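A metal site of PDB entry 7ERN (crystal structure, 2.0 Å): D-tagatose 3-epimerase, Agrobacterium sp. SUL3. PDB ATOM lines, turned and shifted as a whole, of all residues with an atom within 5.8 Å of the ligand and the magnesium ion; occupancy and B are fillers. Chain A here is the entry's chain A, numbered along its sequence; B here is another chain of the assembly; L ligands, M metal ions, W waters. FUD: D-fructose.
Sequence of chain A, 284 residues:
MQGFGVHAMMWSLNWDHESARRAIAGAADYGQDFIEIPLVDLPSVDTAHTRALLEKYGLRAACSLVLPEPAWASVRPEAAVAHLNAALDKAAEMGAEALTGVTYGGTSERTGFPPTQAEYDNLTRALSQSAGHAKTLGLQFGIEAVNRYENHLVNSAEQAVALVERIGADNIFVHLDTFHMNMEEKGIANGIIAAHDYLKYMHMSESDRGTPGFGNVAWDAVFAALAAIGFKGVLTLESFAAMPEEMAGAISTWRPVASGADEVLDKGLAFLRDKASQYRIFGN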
ATOM      1  N   HIS A   7      28.136   4.154  -0.294  1.00  0.00           N
ATOM      2  CA  HIS A   7      27.120   4.091  -1.317  1.00  0.00           C
ATOM      3  C   HIS A   7      26.506   2.693  -1.359  1.00  0.00           C
ATOM      4  O   HIS A   7      27.219   1.684  -1.286  1.00  0.00           O
ATOM      5  CB  HIS A   7      27.737   4.464  -2.672  1.00  0.00           C
ATOM      6  CG  HIS A   7      26.731   4.798  -3.727  1.00  0.00           C
ATOM      7  ND1 HIS A   7      25.826   3.877  -4.216  1.00  0.00           N
ATOM      8  CD2 HIS A   7      26.496   5.952  -4.408  1.00  0.00           C
ATOM      9  CE1 HIS A   7      25.082   4.442  -5.143  1.00  0.00           C
ATOM     10  NE2 HIS A   7      25.459   5.701  -5.282  1.00  0.00           N
ATOM     11  N   MET A   9      25.426   0.994  -3.670  1.00  0.00           N
ATOM     12  CA  MET A   9      25.930   0.195  -4.787  1.00  0.00           C
ATOM     13  C   MET A   9      27.021  -0.791  -4.375  1.00  0.00           C
ATOM     14  O   MET A   9      27.348  -1.689  -5.160  1.00  0.00           O
ATOM     15  CB  MET A   9      26.474   1.120  -5.886  1.00  0.00           C
ATOM     16  CG  MET A   9      27.854   1.748  -5.530  1.00  0.00           C
ATOM     17  SD  MET A   9      28.796   2.520  -6.878  1.00  0.00           S
ATOM     18  CE  MET A   9      27.832   3.989  -7.252  1.00  0.00           C
ATOM     19  N   GLU A  36      24.207   5.981   1.238  1.00  0.00           N
ATOM     20  CA  GLU A  36      23.734   6.746   0.091  1.00  0.00           C
ATOM     21  C   GLU A  36      22.858   5.826  -0.767  1.00  0.00           C
ATOM     22  O   GLU A  36      23.313   4.764  -1.212  1.00  0.00           O
ATOM     23  CB  GLU A  36      24.881   7.308  -0.727  1.00  0.00           C
ATOM     24  CG  GLU A  36      24.394   8.162  -1.862  1.00  0.00           C
ATOM     25  CD  GLU A  36      25.517   8.813  -2.633  1.00  0.00           C
ATOM     26  OE1 GLU A  36      26.530   9.189  -2.000  1.00  0.00           O
ATOM     27  OE2 GLU A  36      25.396   8.954  -3.870  1.00  0.00           O
ATOM     28  N   PRO A  38      20.625   5.220  -4.048  1.00  0.00           N
ATOM     29  CA  PRO A  38      20.322   5.729  -5.383  1.00  0.00           C
ATOM     30  C   PRO A  38      18.846   5.559  -5.697  1.00  0.00           C
ATOM     31  O   PRO A  38      18.210   4.576  -5.307  1.00  0.00           O
ATOM     32  CB  PRO A  38      21.206   4.844  -6.284  1.00  0.00           C
ATOM     33  CG  PRO A  38      21.192   3.515  -5.566  1.00  0.00           C
ATOM     34  CD  PRO A  38      21.102   3.824  -4.072  1.00  0.00           C
ATOM     35  N   LEU A  39      18.274   6.563  -6.353  1.00  0.00           N
ATOM     36  CA  LEU A  39      16.896   6.519  -6.824  1.00  0.00           C
ATOM     37  C   LEU A  39      16.912   6.411  -8.348  1.00  0.00           C
ATOM     38  O   LEU A  39      17.245   7.380  -9.043  1.00  0.00           O
ATOM     39  CB  LEU A  39      16.121   7.770  -6.389  1.00  0.00           C
ATOM     40  CG  LEU A  39      16.095   8.085  -4.893  1.00  0.00           C
ATOM     41  CD1 LEU A  39      15.463   9.433  -4.673  1.00  0.00           C
ATOM     42  CD2 LEU A  39      15.345   7.012  -4.128  1.00  0.00           C
ATOM     43  N   SER A  64      20.549   9.793  -3.936  1.00  0.00           N
ATOM     44  CA  SER A  64      21.235  10.338  -5.094  1.00  0.00           C
ATOM     45  C   SER A  64      20.597   9.821  -6.383  1.00  0.00           C
ATOM     46  O   SER A  64      19.882   8.815  -6.395  1.00  0.00           O
ATOM     47  CB  SER A  64      22.744  10.018  -5.093  1.00  0.00           C
ATOM     48  OG  SER A  64      22.987   8.625  -5.134  1.00  0.00           O
ATOM     49  N   LEU A  65      20.895  10.508  -7.479  1.00  0.00           N
ATOM     50  CA  LEU A  65      20.404  10.084  -8.774  1.00  0.00           C
ATOM     51  C   LEU A  65      21.231  10.724  -9.873  1.00  0.00           C
ATOM     52  O   LEU A  65      22.025  11.650  -9.658  1.00  0.00           O
ATOM     53  CB  LEU A  65      18.922  10.449  -8.967  1.00  0.00           C
ATOM     54  CG  LEU A  65      18.413  11.905  -8.844  1.00  0.00           C
ATOM     55  CD1 LEU A  65      18.879  12.862  -9.946  1.00  0.00           C
ATOM     56  CD2 LEU A  65      16.884  11.860  -8.843  1.00  0.00           C
ATOM     57  N   VAL A  66      21.024  10.192 -11.070  1.00  0.00           N
ATOM     58  CA  VAL A  66      21.375  10.807 -12.347  1.00  0.00           C
ATOM     59  C   VAL A  66      20.065  11.058 -13.091  1.00  0.00           C
ATOM     60  O   VAL A  66      19.194  10.187 -13.121  1.00  0.00           O
ATOM     61  CB  VAL A  66      22.290   9.871 -13.158  1.00  0.00           C
ATOM     62  CG1 VAL A  66      22.608  10.474 -14.509  1.00  0.00           C
ATOM     63  CG2 VAL A  66      23.584   9.546 -12.385  1.00  0.00           C
ATOM     64  N   THR A 100      21.345  14.300  -3.794  1.00  0.00           N
ATOM     65  CA  THR A 100      22.567  14.765  -4.436  1.00  0.00           C
ATOM     66  C   THR A 100      22.830  13.914  -5.682  1.00  0.00           C
ATOM     67  O   THR A 100      21.968  13.144  -6.117  1.00  0.00           O
ATOM     68  CB  THR A 100      23.732  14.725  -3.424  1.00  0.00           C
ATOM     69  OG1 THR A 100      24.875  15.364  -3.974  1.00  0.00           O
ATOM     70  CG2 THR A 100      24.088  13.285  -3.066  1.00  0.00           C
ATOM     71  N   GLY A 101      24.023  14.040  -6.241  1.00  0.00           N
ATOM     72  CA  GLY A 101      24.394  13.322  -7.450  1.00  0.00           C
ATOM     73  C   GLY A 101      24.365  14.222  -8.672  1.00  0.00           C
ATOM     74  O   GLY A 101      24.531  15.438  -8.593  1.00  0.00           O
ATOM     75  N   VAL A 102      24.158  13.586  -9.831  1.00  0.00           N
ATOM     76  CA  VAL A 102      24.107  14.366 -11.062  1.00  0.00           C
ATOM     77  C   VAL A 102      22.676  14.839 -11.244  1.00  0.00           C
ATOM     78  O   VAL A 102      21.921  14.322 -12.076  1.00  0.00           O
ATOM     79  CB  VAL A 102      24.642  13.553 -12.257  1.00  0.00           C
ATOM     80  CG1 VAL A 102      24.801  14.439 -13.488  1.00  0.00           C
ATOM     81  CG2 VAL A 102      26.014  12.954 -11.878  1.00  0.00           C
ATOM     82  N   THR A 107      24.995  11.268 -17.103  1.00  0.00           N
ATOM     83  CA  THR A 107      26.368  10.808 -17.116  1.00  0.00           C
ATOM     84  C   THR A 107      26.763  10.235 -18.467  1.00  0.00           C
ATOM     85  O   THR A 107      27.879   9.723 -18.627  1.00  0.00           O
ATOM     86  CB  THR A 107      26.560   9.762 -16.012  1.00  0.00           C
ATOM     87  OG1 THR A 107      25.516   8.803 -16.095  1.00  0.00           O
ATOM     88  CG2 THR A 107      26.506  10.454 -14.643  1.00  0.00           C
ATOM     89  N   GLU A 144      26.789  17.323  -7.853  1.00  0.00           N
ATOM     90  CA  GLU A 144      28.030  16.553  -7.969  1.00  0.00           C
ATOM     91  C   GLU A 144      28.708  16.847  -9.310  1.00  0.00           C
ATOM     92  O   GLU A 144      28.146  16.555 -10.371  1.00  0.00           O
ATOM     93  CB  GLU A 144      27.801  15.050  -7.819  1.00  0.00           C
ATOM     94  CG  GLU A 144      29.117  14.212  -7.934  1.00  0.00           C
ATOM     95  CD  GLU A 144      28.916  12.714  -7.771  1.00  0.00           C
ATOM     96  OE1 GLU A 144      27.751  12.279  -7.585  1.00  0.00           O
ATOM     97  OE2 GLU A 144      29.928  11.946  -7.851  1.00  0.00           O
ATOM     98  N   VAL A 146      31.102  15.962 -12.264  1.00  0.00           N
ATOM     99  CA  VAL A 146      31.573  14.734 -12.870  1.00  0.00           C
ATOM    100  C   VAL A 146      32.523  15.077 -14.008  1.00  0.00           C
ATOM    101  O   VAL A 146      32.646  16.228 -14.402  1.00  0.00           O
ATOM    102  CB  VAL A 146      30.417  13.843 -13.348  1.00  0.00           C
ATOM    103  CG1 VAL A 146      29.534  13.452 -12.171  1.00  0.00           C
ATOM    104  CG2 VAL A 146      29.584  14.576 -14.414  1.00  0.00           C
ATOM    105  N   GLU A 150      31.388  12.320 -18.945  1.00  0.00           N
ATOM    106  CA  GLU A 150      30.035  12.006 -18.523  1.00  0.00           C
ATOM    107  C   GLU A 150      29.083  13.165 -18.764  1.00  0.00           C
ATOM    108  O   GLU A 150      27.869  12.944 -18.956  1.00  0.00           O
ATOM    109  CB  GLU A 150      30.038  11.639 -17.030  1.00  0.00           C
ATOM    110  CG  GLU A 150      30.807  10.356 -16.781  1.00  0.00           C
ATOM    111  CD  GLU A 150      30.589   9.808 -15.390  1.00  0.00           C
ATOM    112  OE1 GLU A 150      29.809  10.430 -14.628  1.00  0.00           O
ATOM    113  OE2 GLU A 150      31.184   8.761 -15.061  1.00  0.00           O
ATOM    114  N   HIS A 175      29.114  18.884  -4.182  1.00  0.00           N
ATOM    115  CA  HIS A 175      29.439  17.487  -3.920  1.00  0.00           C
ATOM    116  C   HIS A 175      30.566  17.142  -4.880  1.00  0.00           C
ATOM    117  O   HIS A 175      30.385  17.251  -6.098  1.00  0.00           O
ATOM    118  CB  HIS A 175      28.176  16.627  -4.150  1.00  0.00           C
ATOM    119  CG  HIS A 175      28.375  15.146  -4.143  1.00  0.00           C
ATOM    120  ND1 HIS A 175      27.324  14.266  -4.285  1.00  0.00           N
ATOM    121  CD2 HIS A 175      29.489  14.379  -4.027  1.00  0.00           C
ATOM    122  CE1 HIS A 175      27.776  13.023  -4.266  1.00  0.00           C
ATOM    123  NE2 HIS A 175      29.093  13.067  -4.106  1.00  0.00           N
ATOM    124  N   ASP A 177      33.757  14.446  -6.207  1.00  0.00           N
ATOM    125  CA  ASP A 177      34.045  13.020  -6.349  1.00  0.00           C
ATOM    126  C   ASP A 177      35.508  12.898  -6.739  1.00  0.00           C
ATOM    127  O   ASP A 177      35.909  13.449  -7.772  1.00  0.00           O
ATOM    128  CB  ASP A 177      33.103  12.384  -7.381  1.00  0.00           C
ATOM    129  CG  ASP A 177      33.341  10.882  -7.561  1.00  0.00           C
ATOM    130  OD1 ASP A 177      34.504  10.441  -7.491  1.00  0.00           O
ATOM    131  OD2 ASP A 177      32.353  10.140  -7.797  1.00  0.00           O
ATOM    132  N   HIS A 180      36.376  11.759 -10.236  1.00  0.00           N
ATOM    133  CA  HIS A 180      36.232  12.778 -11.263  1.00  0.00           C
ATOM    134  C   HIS A 180      37.263  13.884 -11.111  1.00  0.00           C
ATOM    135  O   HIS A 180      37.777  14.409 -12.110  1.00  0.00           O
ATOM    136  CB  HIS A 180      34.828  13.349 -11.203  1.00  0.00           C
ATOM    137  CG  HIS A 180      33.756  12.337 -11.506  1.00  0.00           C
ATOM    138  ND1 HIS A 180      33.733  11.622 -12.685  1.00  0.00           N
ATOM    139  CD2 HIS A 180      32.679  11.947 -10.794  1.00  0.00           C
ATOM    140  CE1 HIS A 180      32.681  10.819 -12.677  1.00  0.00           C
ATOM    141  NE2 HIS A 180      32.020  10.994 -11.546  1.00  0.00           N
ATOM    142  N   HIS A 203      32.343  12.063  -2.567  1.00  0.00           N
ATOM    143  CA  HIS A 203      32.542  10.672  -2.938  1.00  0.00           C
ATOM    144  C   HIS A 203      34.038  10.391  -2.873  1.00  0.00           C
ATOM    145  O   HIS A 203      34.825  10.954  -3.637  1.00  0.00           O
ATOM    146  CB  HIS A 203      31.973  10.365  -4.316  1.00  0.00           C
ATOM    147  CG  HIS A 203      30.495  10.085  -4.295  1.00  0.00           C
ATOM    148  ND1 HIS A 203      29.739   9.998  -5.439  1.00  0.00           N
ATOM    149  CD2 HIS A 203      29.649   9.873  -3.255  1.00  0.00           C
ATOM    150  CE1 HIS A 203      28.478   9.740  -5.099  1.00  0.00           C
ATOM    151  NE2 HIS A 203      28.407   9.664  -3.789  1.00  0.00           N
ATOM    152  N   ARG A 209      38.001   3.449  -9.645  1.00  0.00           N
ATOM    153  CA  ARG A 209      36.762   3.030  -9.000  1.00  0.00           C
ATOM    154  C   ARG A 209      36.953   1.753  -8.208  1.00  0.00           C
ATOM    155  O   ARG A 209      35.969   1.095  -7.864  1.00  0.00           O
ATOM    156  CB  ARG A 209      35.613   2.844 -10.009  1.00  0.00           C
ATOM    157  CG  ARG A 209      35.188   4.139 -10.703  1.00  0.00           C
ATOM    158  CD  ARG A 209      34.524   5.083  -9.703  1.00  0.00           C
ATOM    159  NE  ARG A 209      33.619   6.005 -10.359  1.00  0.00           N
ATOM    160  CZ  ARG A 209      33.088   7.087  -9.782  1.00  0.00           C
ATOM    161  NH1 ARG A 209      33.386   7.392  -8.518  1.00  0.00           N
ATOM    162  NH2 ARG A 209      32.247   7.861 -10.464  1.00  0.00           N
ATOM    163  N   GLU A 238      32.631   5.395  -2.668  1.00  0.00           N
ATOM    164  CA  GLU A 238      32.024   4.957  -3.925  1.00  0.00           C
ATOM    165  C   GLU A 238      33.025   4.077  -4.647  1.00  0.00           C
ATOM    166  O   GLU A 238      34.157   4.500  -4.907  1.00  0.00           O
ATOM    167  CB  GLU A 238      31.624   6.171  -4.776  1.00  0.00           C
ATOM    168  CG  GLU A 238      31.171   5.848  -6.204  1.00  0.00           C
ATOM    169  CD  GLU A 238      30.302   6.964  -6.763  1.00  0.00           C
ATOM    170  OE1 GLU A 238      29.059   6.811  -6.782  1.00  0.00           O
ATOM    171  OE2 GLU A 238      30.849   8.019  -7.142  1.00  0.00           O
ATOM    172  N   PHE A 240      33.048   0.563  -7.669  1.00  0.00           N
ATOM    173  CA  PHE A 240      32.237  -0.256  -8.571  1.00  0.00           C
ATOM    174  C   PHE A 240      32.425  -1.760  -8.350  1.00  0.00           C
ATOM    175  O   PHE A 240      31.971  -2.565  -9.176  1.00  0.00           O
ATOM    176  CB  PHE A 240      32.518   0.124 -10.030  1.00  0.00           C
ATOM    177  CG  PHE A 240      31.946   1.459 -10.443  1.00  0.00           C
ATOM    178  CD1 PHE A 240      31.122   2.178  -9.596  1.00  0.00           C
ATOM    179  CD2 PHE A 240      32.220   1.980 -11.703  1.00  0.00           C
ATOM    180  CE1 PHE A 240      30.587   3.416  -9.991  1.00  0.00           C
ATOM    181  CE2 PHE A 240      31.702   3.202 -12.092  1.00  0.00           C
ATOM    182  CZ  PHE A 240      30.875   3.915 -11.238  1.00  0.00           C
ATOM    183  N   TYR B 149      36.169   5.590 -21.258  1.00  0.00           N
ATOM    184  CA  TYR B 149      35.165   6.444 -21.884  1.00  0.00           C
ATOM    185  C   TYR B 149      35.394   6.625 -23.384  1.00  0.00           C
ATOM    186  O   TYR B 149      34.458   7.027 -24.098  1.00  0.00           O
ATOM    187  CB  TYR B 149      35.155   7.814 -21.225  1.00  0.00           C
ATOM    188  CG  TYR B 149      34.666   7.818 -19.807  1.00  0.00           C
ATOM    189  CD1 TYR B 149      33.297   7.794 -19.510  1.00  0.00           C
ATOM    190  CD2 TYR B 149      35.579   7.872 -18.750  1.00  0.00           C
ATOM    191  CE1 TYR B 149      32.853   7.822 -18.204  1.00  0.00           C
ATOM    192  CE2 TYR B 149      35.144   7.899 -17.441  1.00  0.00           C
ATOM    193  CZ  TYR B 149      33.787   7.882 -17.186  1.00  0.00           C
ATOM    194  OH  TYR B 149      33.363   7.900 -15.880  1.00  0.00           O
HETATM  195  C1  FUD L   1      28.606   8.908 -11.403  1.00  0.00           C
HETATM  196  C2  FUD L   1      28.948   9.101  -9.932  1.00  0.00           C
HETATM  197  C3  FUD L   1      27.879   8.903  -8.870  1.00  0.00           C
HETATM  198  C4  FUD L   1      26.449   9.110  -9.350  1.00  0.00           C
HETATM  199  C5  FUD L   1      25.539   8.561  -8.251  1.00  0.00           C
HETATM  200  C6  FUD L   1      24.046   8.696  -8.573  1.00  0.00           C
HETATM  201  O1  FUD L   1      29.534   9.667 -12.109  1.00  0.00           O
HETATM  202  O2  FUD L   1      30.063   9.377  -9.589  1.00  0.00           O
HETATM  203  O3  FUD L   1      28.150   9.860  -7.887  1.00  0.00           O
HETATM  204  O4  FUD L   1      26.208  10.470  -9.518  1.00  0.00           O
HETATM  205  O5  FUD L   1      25.883   7.216  -8.073  1.00  0.00           O
HETATM  206  O6  FUD L   1      23.271   7.809  -7.791  1.00  0.00           O
HETATM  207 MG    MG M   1      30.346  10.001  -7.544  1.00  0.00          MG
HETATM  208  O   HOH W   1      26.273   5.372 -10.473  1.00  0.00           O
HETATM  209  O   HOH W   2      21.699   6.398  -9.086  1.00  0.00           O
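A ring nitrogen (NE2) of His 180 sits at hydrogen-bond distance from an oxygen (O1) of the ligand, at 2.9 Å. The side-chain hydroxyl (OG) of Ser 64 sits at hydrogen-bond distance from an oxygen (O6) of the ligand, at 2.8 Å. OE1 of Glu 150 sits at hydrogen-bond distance from O1 of the ligand. The guanidinium group (NH2) of Arg 209 sits close to an oxygen (O2) of the ligand (2.8 Å). NE2 of His 7 lies within hydrogen-bond range of O5 of the ligand, 3.2 Å away.
Four residues have an atom within 4 Å of the magnesium ion: Glu 144, Asp 177, His 203 and Glu 238. Along chain A the residues within 4 Å of the magnesium ion span positions 144 to 238. The nearest printed residue that does not touch the magnesium ion is Arg 209 (4.1 Å).
Met 9 touches the ligand. Pro 38 touches the ligand. Leu 65 touches the ligand. Val 66 touches the ligand. CA of Gly 101 touches O4 of the ligand, at 3.96 Å. CG2 of Val 102 touches O4 of the ligand (3.4 Å). Val 146 touches the ligand. Hydrophobic or aromatic side chains that line the ligand: His 7, Met 9, Pro 38, Val 66, Val 102, Val 146, His 180 and His 203. Of the 23 residues printed, 16 come within 4 Å of the ligand. The nearest printed residue that does not touch the ligand is Thr 107 (4.03 Å).
The magnesium ion is bound by the side-chain carboxylate (OE2) of Glu 144 (2.0 Å), the side-chain carboxylate (OD2) of Asp 177 (2.0 Å), the side-chain carboxylate (OE2) of Glu 238 (2.1 Å), an oxygen (O2) of the ligand (2.2 Å), a ring nitrogen (ND1) of His 203 (2.2 Å) and an oxygen (O3) of the ligand (2.2 Å).
The backbone NH (N) of Met 9 is in hydrogen-bond range of a ring nitrogen (ND1) of His 7 (3.0 Å). N of Leu 65 sits at hydrogen-bond distance from O of Thr 100 (3.2 Å). OE2 of Glu 238 sits close to NH1 of Arg 209 (3.0 Å). A ring nitrogen (NE2) of His 203 sits close to a ring nitrogen (NE2) of His 175, 3.5 Å away. The backbone NH (N) of Glu 144 sits at hydrogen-bond distance from the backbone carbonyl oxygen (O) of Gly 101 (3.0 Å). The backbone carbonyl oxygen of Leu 65 lies within hydrogen-bond range of the backbone NH of Val 102, 2.9 Å away. O of Ser 64 is in hydrogen-bond range of N of Leu 39 (2.8 Å). O of Arg 209 lies within hydrogen-bond range of N of Phe 240, at 3.0 Å.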
